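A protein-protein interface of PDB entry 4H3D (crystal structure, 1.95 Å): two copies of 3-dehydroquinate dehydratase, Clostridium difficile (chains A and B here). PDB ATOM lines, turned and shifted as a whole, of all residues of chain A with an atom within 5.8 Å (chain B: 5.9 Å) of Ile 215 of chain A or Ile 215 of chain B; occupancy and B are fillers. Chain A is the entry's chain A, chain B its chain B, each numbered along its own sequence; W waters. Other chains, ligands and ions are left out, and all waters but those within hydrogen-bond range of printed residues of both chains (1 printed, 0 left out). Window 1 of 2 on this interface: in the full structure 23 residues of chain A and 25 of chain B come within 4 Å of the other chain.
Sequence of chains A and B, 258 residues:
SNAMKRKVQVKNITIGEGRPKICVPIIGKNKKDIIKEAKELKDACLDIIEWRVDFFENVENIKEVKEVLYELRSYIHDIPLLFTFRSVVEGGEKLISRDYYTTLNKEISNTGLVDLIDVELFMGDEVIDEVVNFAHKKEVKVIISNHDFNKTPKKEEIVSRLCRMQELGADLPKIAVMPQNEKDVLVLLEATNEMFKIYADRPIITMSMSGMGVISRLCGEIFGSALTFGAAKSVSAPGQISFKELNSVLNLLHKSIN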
ATOM      1  N   VAL A 185      31.187 -10.307   3.811  1.00  0.00           N
ATOM      2  CA  VAL A 185      30.065  -9.695   4.522  1.00  0.00           C
ATOM      3  C   VAL A 185      28.887  -9.545   3.545  1.00  0.00           C
ATOM      4  O   VAL A 185      27.727  -9.782   3.905  1.00  0.00           O
ATOM      5  CB  VAL A 185      30.434  -8.313   5.121  1.00  0.00           C
ATOM      6  CG1 VAL A 185      29.246  -7.695   5.795  1.00  0.00           C
ATOM      7  CG2 VAL A 185      31.622  -8.449   6.110  1.00  0.00           C
ATOM      8  N   LEU A 189      25.014 -11.158   3.482  1.00  0.00           N
ATOM      9  CA  LEU A 189      23.804 -10.345   3.234  1.00  0.00           C
ATOM     10  C   LEU A 189      23.024 -10.818   1.985  1.00  0.00           C
ATOM     11  O   LEU A 189      21.799 -10.857   1.996  1.00  0.00           O
ATOM     12  CB  LEU A 189      24.157  -8.855   3.116  1.00  0.00           C
ATOM     13  CG  LEU A 189      24.677  -8.179   4.420  1.00  0.00           C
ATOM     14  CD1 LEU A 189      25.104  -6.705   4.202  1.00  0.00           C
ATOM     15  CD2 LEU A 189      23.613  -8.259   5.508  1.00  0.00           C
ATOM     16  N   GLY A 211      34.277  -7.264  13.817  1.00  0.00           N
ATOM     17  CA  GLY A 211      34.103  -5.840  13.528  1.00  0.00           C
ATOM     18  C   GLY A 211      33.722  -5.583  12.083  1.00  0.00           C
ATOM     19  O   GLY A 211      32.918  -4.711  11.794  1.00  0.00           O
ATOM     20  N   MET A 212      34.288  -6.354  11.164  1.00  0.00           N
ATOM     21  CA  MET A 212      33.978  -6.187   9.737  1.00  0.00           C
ATOM     22  C   MET A 212      32.492  -6.468   9.400  1.00  0.00           C
ATOM     23  O   MET A 212      31.930  -5.857   8.483  1.00  0.00           O
ATOM     24  CB  MET A 212      34.889  -7.110   8.921  1.00  0.00           C
ATOM     25  CG  MET A 212      34.980  -6.803   7.463  1.00  0.00           C
ATOM     26  SD  MET A 212      36.258  -7.809   6.661  1.00  0.00           S
ATOM     27  CE  MET A 212      37.733  -7.225   7.472  1.00  0.00           C
ATOM     28  N   GLY A 213      31.852  -7.381  10.139  1.00  0.00           N
ATOM     29  CA  GLY A 213      30.436  -7.748   9.855  1.00  0.00           C
ATOM     30  C   GLY A 213      29.364  -6.996  10.640  1.00  0.00           C
ATOM     31  O   GLY A 213      28.170  -7.274  10.484  1.00  0.00           O
ATOM     32  N   VAL A 214      29.773  -6.028  11.447  1.00  0.00           N
ATOM     33  CA  VAL A 214      28.836  -5.312  12.334  1.00  0.00           C
ATOM     34  C   VAL A 214      27.658  -4.701  11.587  1.00  0.00           C
ATOM     35  O   VAL A 214      26.517  -4.672  12.096  1.00  0.00           O
ATOM     36  CB  VAL A 214      29.569  -4.269  13.225  1.00  0.00           C
ATOM     37  CG1 VAL A 214      28.570  -3.334  13.927  1.00  0.00           C
ATOM     38  CG2 VAL A 214      30.435  -4.983  14.262  1.00  0.00           C
ATOM     39  N   ILE A 215      27.899  -4.263  10.361  1.00  0.00           N
ATOM     40  CA  ILE A 215      26.833  -3.708   9.548  1.00  0.00           C
ATOM     41  C   ILE A 215      25.643  -4.704   9.393  1.00  0.00           C
ATOM     42  O   ILE A 215      24.462  -4.275   9.331  1.00  0.00           O
ATOM     43  CB  ILE A 215      27.384  -3.211   8.176  1.00  0.00           C
ATOM     44  CG1 ILE A 215      26.371  -2.300   7.483  1.00  0.00           C
ATOM     45  CG2 ILE A 215      27.823  -4.402   7.297  1.00  0.00           C
ATOM     46  CD1 ILE A 215      26.103  -0.974   8.233  1.00  0.00           C
ATOM     47  N   SER A 216      25.938  -6.023   9.383  1.00  0.00           N
ATOM     48  CA  SER A 216      24.911  -7.079   9.266  1.00  0.00           C
ATOM     49  C   SER A 216      23.960  -7.119  10.467  1.00  0.00           C
ATOM     50  O   SER A 216      22.888  -7.721  10.391  1.00  0.00           O
ATOM     51  CB  SER A 216      25.558  -8.485   9.104  1.00  0.00           C
ATOM     52  OG  SER A 216      26.238  -8.925  10.291  1.00  0.00           O
ATOM     53  N   ARG A 217      24.351  -6.512  11.582  1.00  0.00           N
ATOM     54  CA  ARG A 217      23.496  -6.477  12.765  1.00  0.00           C
ATOM     55  C   ARG A 217      22.549  -5.297  12.718  1.00  0.00           C
ATOM     56  O   ARG A 217      21.618  -5.203  13.523  1.00  0.00           O
ATOM     57  CB  ARG A 217      24.331  -6.351  14.033  1.00  0.00           C
ATOM     58  CG  ARG A 217      25.360  -7.427  14.214  1.00  0.00           C
ATOM     59  CD  ARG A 217      26.194  -7.177  15.432  1.00  0.00           C
ATOM     60  NE  ARG A 217      27.253  -8.184  15.574  1.00  0.00           N
ATOM     61  CZ  ARG A 217      27.141  -9.300  16.277  1.00  0.00           C
ATOM     62  NH1 ARG A 217      26.014  -9.575  16.930  1.00  0.00           N
ATOM     63  NH2 ARG A 217      28.163 -10.140  16.341  1.00  0.00           N
ATOM     64  N   LEU A 218      22.780  -4.384  11.790  1.00  0.00           N
ATOM     65  CA  LEU A 218      21.986  -3.164  11.732  1.00  0.00           C
ATOM     66  C   LEU A 218      20.954  -3.105  10.623  1.00  0.00           C
ATOM     67  O   LEU A 218      19.931  -2.439  10.770  1.00  0.00           O
ATOM     68  CB  LEU A 218      22.922  -1.949  11.564  1.00  0.00           C
ATOM     69  CG  LEU A 218      24.059  -1.716  12.575  1.00  0.00           C
ATOM     70  CD1 LEU A 218      24.738  -0.382  12.306  1.00  0.00           C
ATOM     71  CD2 LEU A 218      23.559  -1.743  14.006  1.00  0.00           C
ATOM     72  N   CYS A 219      21.196  -3.832   9.528  1.00  0.00           N
ATOM     73  CA  CYS A 219      20.348  -3.727   8.319  1.00  0.00           C
ATOM     74  C   CYS A 219      19.369  -4.875   8.074  1.00  0.00           C
ATOM     75  O   CYS A 219      18.948  -5.101   6.938  1.00  0.00           O
ATOM     76  CB  CYS A 219      21.258  -3.598   7.092  1.00  0.00           C
ATOM     77  SG  CYS A 219      22.259  -5.084   6.776  1.00  0.00           S
ATOM     78  N   GLY A 220      18.959  -5.560   9.129  1.00  0.00           N
ATOM     79  CA  GLY A 220      18.063  -6.711   8.987  1.00  0.00           C
ATOM     80  C   GLY A 220      16.688  -6.445   8.378  1.00  0.00           C
ATOM     81  O   GLY A 220      16.102  -7.324   7.756  1.00  0.00           O
ATOM     82  N   PHE A 223      17.485  -6.421   4.496  1.00  0.00           N
ATOM     83  CA  PHE A 223      17.966  -7.667   3.917  1.00  0.00           C
ATOM     84  C   PHE A 223      17.259  -8.948   4.342  1.00  0.00           C
ATOM     85  O   PHE A 223      17.285  -9.929   3.605  1.00  0.00           O
ATOM     86  CB  PHE A 223      19.477  -7.738   4.021  1.00  0.00           C
ATOM     87  CG  PHE A 223      20.164  -6.627   3.256  1.00  0.00           C
ATOM     88  CD1 PHE A 223      20.274  -6.687   1.885  1.00  0.00           C
ATOM     89  CD2 PHE A 223      20.642  -5.508   3.908  1.00  0.00           C
ATOM     90  CE1 PHE A 223      20.878  -5.659   1.165  1.00  0.00           C
ATOM     91  CE2 PHE A 223      21.249  -4.479   3.205  1.00  0.00           C
ATOM     92  CZ  PHE A 223      21.368  -4.562   1.824  1.00  0.00           C
ATOM     93  N   VAL B 185      21.904  -2.910  -4.126  1.00  0.00           N
ATOM     94  CA  VAL B 185      22.594  -2.204  -3.025  1.00  0.00           C
ATOM     95  C   VAL B 185      23.930  -2.900  -2.774  1.00  0.00           C
ATOM     96  O   VAL B 185      24.975  -2.242  -2.640  1.00  0.00           O
ATOM     97  CB  VAL B 185      21.787  -2.209  -1.746  1.00  0.00           C
ATOM     98  CG1 VAL B 185      22.560  -1.488  -0.632  1.00  0.00           C
ATOM     99  CG2 VAL B 185      20.416  -1.564  -1.947  1.00  0.00           C
ATOM    100  N   LEU B 186      23.902  -4.235  -2.733  1.00  0.00           N
ATOM    101  CA  LEU B 186      25.118  -5.007  -2.512  1.00  0.00           C
ATOM    102  C   LEU B 186      26.119  -4.829  -3.669  1.00  0.00           C
ATOM    103  O   LEU B 186      27.330  -4.777  -3.447  1.00  0.00           O
ATOM    104  CB  LEU B 186      24.785  -6.495  -2.262  1.00  0.00           C
ATOM    105  CG  LEU B 186      23.871  -6.783  -1.046  1.00  0.00           C
ATOM    106  CD1 LEU B 186      23.621  -8.269  -0.881  1.00  0.00           C
ATOM    107  CD2 LEU B 186      24.467  -6.212   0.243  1.00  0.00           C
ATOM    108  N   LEU B 189      27.981  -1.664  -3.148  1.00  0.00           N
ATOM    109  CA  LEU B 189      28.982  -1.894  -2.095  1.00  0.00           C
ATOM    110  C   LEU B 189      30.155  -2.753  -2.585  1.00  0.00           C
ATOM    111  O   LEU B 189      31.313  -2.489  -2.238  1.00  0.00           O
ATOM    112  CB  LEU B 189      28.335  -2.515  -0.847  1.00  0.00           C
ATOM    113  CG  LEU B 189      27.358  -1.614  -0.070  1.00  0.00           C
ATOM    114  CD1 LEU B 189      26.792  -2.379   1.139  1.00  0.00           C
ATOM    115  CD2 LEU B 189      28.030  -0.310   0.385  1.00  0.00           C
ATOM    116  N   GLY B 211      15.457   4.327   0.446  1.00  0.00           N
ATOM    117  CA  GLY B 211      15.438   3.668   1.780  1.00  0.00           C
ATOM    118  C   GLY B 211      16.235   2.387   1.783  1.00  0.00           C
ATOM    119  O   GLY B 211      16.975   2.096   2.710  1.00  0.00           O
ATOM    120  N   MET B 212      16.094   1.635   0.707  1.00  0.00           N
ATOM    121  CA  MET B 212      16.790   0.376   0.519  1.00  0.00           C
ATOM    122  C   MET B 212      18.322   0.541   0.523  1.00  0.00           C
ATOM    123  O   MET B 212      19.043  -0.358   0.954  1.00  0.00           O
ATOM    124  CB  MET B 212      16.319  -0.216  -0.827  1.00  0.00           C
ATOM    125  CG  MET B 212      16.813  -1.580  -1.184  1.00  0.00           C
ATOM    126  SD  MET B 212      16.010  -2.191  -2.711  1.00  0.00           S
ATOM    127  CE  MET B 212      14.328  -2.369  -2.148  1.00  0.00           C
ATOM    128  N   GLY B 213      18.818   1.696   0.063  1.00  0.00           N
ATOM    129  CA  GLY B 213      20.258   1.906  -0.056  1.00  0.00           C
ATOM    130  C   GLY B 213      20.968   2.556   1.121  1.00  0.00           C
ATOM    131  O   GLY B 213      22.175   2.753   1.065  1.00  0.00           O
ATOM    132  N   VAL B 214      20.236   2.844   2.192  1.00  0.00           N
ATOM    133  CA  VAL B 214      20.793   3.577   3.356  1.00  0.00           C
ATOM    134  C   VAL B 214      22.051   2.960   3.967  1.00  0.00           C
ATOM    135  O   VAL B 214      22.930   3.692   4.425  1.00  0.00           O
ATOM    136  CB  VAL B 214      19.730   3.791   4.438  1.00  0.00           C
ATOM    137  CG1 VAL B 214      20.350   4.404   5.695  1.00  0.00           C
ATOM    138  CG2 VAL B 214      18.615   4.679   3.891  1.00  0.00           C
ATOM    139  N   ILE B 215      22.153   1.633   3.970  1.00  0.00           N
ATOM    140  CA  ILE B 215      23.360   0.972   4.476  1.00  0.00           C
ATOM    141  C   ILE B 215      24.601   1.571   3.837  1.00  0.00           C
ATOM    142  O   ILE B 215      25.664   1.689   4.479  1.00  0.00           O
ATOM    143  CB  ILE B 215      23.336  -0.584   4.196  1.00  0.00           C
ATOM    144  CG1 ILE B 215      24.611  -1.270   4.724  1.00  0.00           C
ATOM    145  CG2 ILE B 215      23.179  -0.881   2.695  1.00  0.00           C
ATOM    146  CD1 ILE B 215      24.675  -2.805   4.434  1.00  0.00           C
ATOM    147  N   SER B 216      24.471   1.958   2.565  1.00  0.00           N
ATOM    148  CA  SER B 216      25.591   2.513   1.824  1.00  0.00           C
ATOM    149  C   SER B 216      26.068   3.848   2.400  1.00  0.00           C
ATOM    150  O   SER B 216      27.171   4.289   2.074  1.00  0.00           O
ATOM    151  CB  SER B 216      25.235   2.699   0.360  1.00  0.00           C
ATOM    152  OG  SER B 216      24.297   3.752   0.191  1.00  0.00           O
ATOM    153  N   ARG B 217      25.234   4.488   3.217  1.00  0.00           N
ATOM    154  CA  ARG B 217      25.582   5.768   3.846  1.00  0.00           C
ATOM    155  C   ARG B 217      26.234   5.542   5.191  1.00  0.00           C
ATOM    156  O   ARG B 217      26.813   6.476   5.773  1.00  0.00           O
ATOM    157  CB  ARG B 217      24.340   6.617   4.101  1.00  0.00           C
ATOM    158  CG  ARG B 217      23.559   6.936   2.881  1.00  0.00           C
ATOM    159  CD  ARG B 217      22.390   7.849   3.200  1.00  0.00           C
ATOM    160  NE  ARG B 217      21.597   8.107   2.000  1.00  0.00           N
ATOM    161  CZ  ARG B 217      21.727   9.170   1.207  1.00  0.00           C
ATOM    162  NH1 ARG B 217      22.620  10.122   1.478  1.00  0.00           N
ATOM    163  NH2 ARG B 217      20.947   9.288   0.146  1.00  0.00           N
ATOM    164  N   LEU B 218      26.134   4.310   5.692  1.00  0.00           N
ATOM    165  CA  LEU B 218      26.609   3.997   7.037  1.00  0.00           C
ATOM    166  C   LEU B 218      27.916   3.251   7.085  1.00  0.00           C
ATOM    167  O   LEU B 218      28.660   3.402   8.045  1.00  0.00           O
ATOM    168  CB  LEU B 218      25.565   3.121   7.763  1.00  0.00           C
ATOM    169  CG  LEU B 218      24.119   3.623   7.846  1.00  0.00           C
ATOM    170  CD1 LEU B 218      23.259   2.628   8.597  1.00  0.00           C
ATOM    171  CD2 LEU B 218      24.059   4.981   8.534  1.00  0.00           C
ATOM    172  N   CYS B 219      28.198   2.461   6.056  1.00  0.00           N
ATOM    173  CA  CYS B 219      29.307   1.507   6.102  1.00  0.00           C
ATOM    174  C   CYS B 219      30.562   1.883   5.322  1.00  0.00           C
ATOM    175  O   CYS B 219      31.322   1.004   4.908  1.00  0.00           O
ATOM    176  CB  CYS B 219      28.798   0.152   5.605  1.00  0.00           C
ATOM    177  SG  CYS B 219      28.352   0.187   3.864  1.00  0.00           S
ATOM    178  N   GLY B 220      30.795   3.174   5.140  1.00  0.00           N
ATOM    179  CA  GLY B 220      31.965   3.643   4.421  1.00  0.00           C
ATOM    180  C   GLY B 220      33.301   3.196   4.977  1.00  0.00           C
ATOM    181  O   GLY B 220      34.225   2.881   4.217  1.00  0.00           O
ATOM    182  N   PHE B 223      33.591  -0.557   3.724  1.00  0.00           N
ATOM    183  CA  PHE B 223      33.586  -0.804   2.283  1.00  0.00           C
ATOM    184  C   PHE B 223      34.378   0.177   1.430  1.00  0.00           C
ATOM    185  O   PHE B 223      34.801  -0.170   0.336  1.00  0.00           O
ATOM    186  CB  PHE B 223      32.158  -1.017   1.796  1.00  0.00           C
ATOM    187  CG  PHE B 223      31.538  -2.240   2.380  1.00  0.00           C
ATOM    188  CD1 PHE B 223      31.814  -3.486   1.848  1.00  0.00           C
ATOM    189  CD2 PHE B 223      30.765  -2.165   3.518  1.00  0.00           C
ATOM    190  CE1 PHE B 223      31.277  -4.626   2.413  1.00  0.00           C
ATOM    191  CE2 PHE B 223      30.221  -3.314   4.086  1.00  0.00           C
ATOM    192  CZ  PHE B 223      30.481  -4.531   3.534  1.00  0.00           C
ATOM    193  N   LEU B 253      30.172   2.440  14.577  1.00  0.00           N
ATOM    194  CA  LEU B 253      30.891   1.516  13.680  1.00  0.00           C
ATOM    195  C   LEU B 253      32.417   1.701  13.756  1.00  0.00           C
ATOM    196  O   LEU B 253      33.169   0.728  13.620  1.00  0.00           O
ATOM    197  CB  LEU B 253      30.388   1.638  12.227  1.00  0.00           C
ATOM    198  CG  LEU B 253      28.927   1.198  11.993  1.00  0.00           C
ATOM    199  CD1 LEU B 253      28.383   1.627  10.603  1.00  0.00           C
ATOM    200  CD2 LEU B 253      28.765  -0.286  12.176  1.00  0.00           C
HETATM  201  O   HOH W   1      32.387  -2.108  11.847  1.00  0.00           O
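Leu 189 of chain A touches Ile 215 of chain B, but with the chains exchanged Ile 215 of chain A does not touch Leu 189 of chain B (6.4 Å). Ile 215 of chain A touches its own counterpart, Ile 215 of chain B. Ile 215 of chain A touches Cys 219 of chain B, but with the chains exchanged Cys 219 of chain A does not touch Ile 215 of chain B (4.1 Å). Of the 6 pairs that touch across the chains among the printed residues, 1 has its exchanged pair printed and touching as well.
Among the printed residues, pairs that only touch across the chains: Ile 215 of chain A with Ile 215 of chain B, Val 214 of chain A with Leu 253 of chain B, Phe 223 of chain A with Leu 186 of chain B, Leu 189 of chain A with Leu 186 of chain B, Ile 215 of chain A with Cys 219 of chain B and Leu 189 of chain A with Ile 215 of chain B.
Water W1 lies within hydrogen-bond range of the backbone carbonyl oxygen of Gly 211 of chain A (2.7 Å) and the backbone carbonyl oxygen of Leu 253 of chain B (3.4 Å).
Of the 13 printed residues of chain A, 4 touch a printed residue of chain B. Printed residues of chain B that touch a printed residue of chain A: Leu 186, Ile 215, Cys 219 and Leu 253. Among the printed residues, no Asp or Glu carboxylate lies within 4 Å of a Lys or Arg side-chain nitrogen of the other chain.
The backbone carbonyl oxygen (O) of Ile 215 of chain A is in hydrogen-bond range of the side-chain sulfur (SG) of Cys 219 of chain A, at 3.5 Å. SG of Cys 219 of chain B is in hydrogen-bond range of O of Ile 215 of chain B.
Ile 215 of chain A touches just these residues of chain B: Ile 215 (3.4 Å) and Cys 219 (3.9 Å). Printed residues of chain A within 4 Å of Ile 215 of chain B: Leu 189 and Ile 215. Of the printed residues of chain B, Phe 223 of chain A touches Leu 186 (3.7 Å). Of the printed residues of chain B, Val 214 of chain A touches Leu 253. Gly 213 of chain B touches none of the printed residues of chain A. Gly 213 of chain A touches none of the printed residues of chain B. The nearest printed residue of chain B that does not touch Ile 215 of chain A is Phe 223 of chain B (4.2 Å). The nearest printed residue of chain A that does not touch Ile 215 of chain B is Phe 223 of chain A (4.01 Å). The nearest printed residue of chain B that does not touch Leu 189 of chain A is Leu 189 of chain B (5.6 Å).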
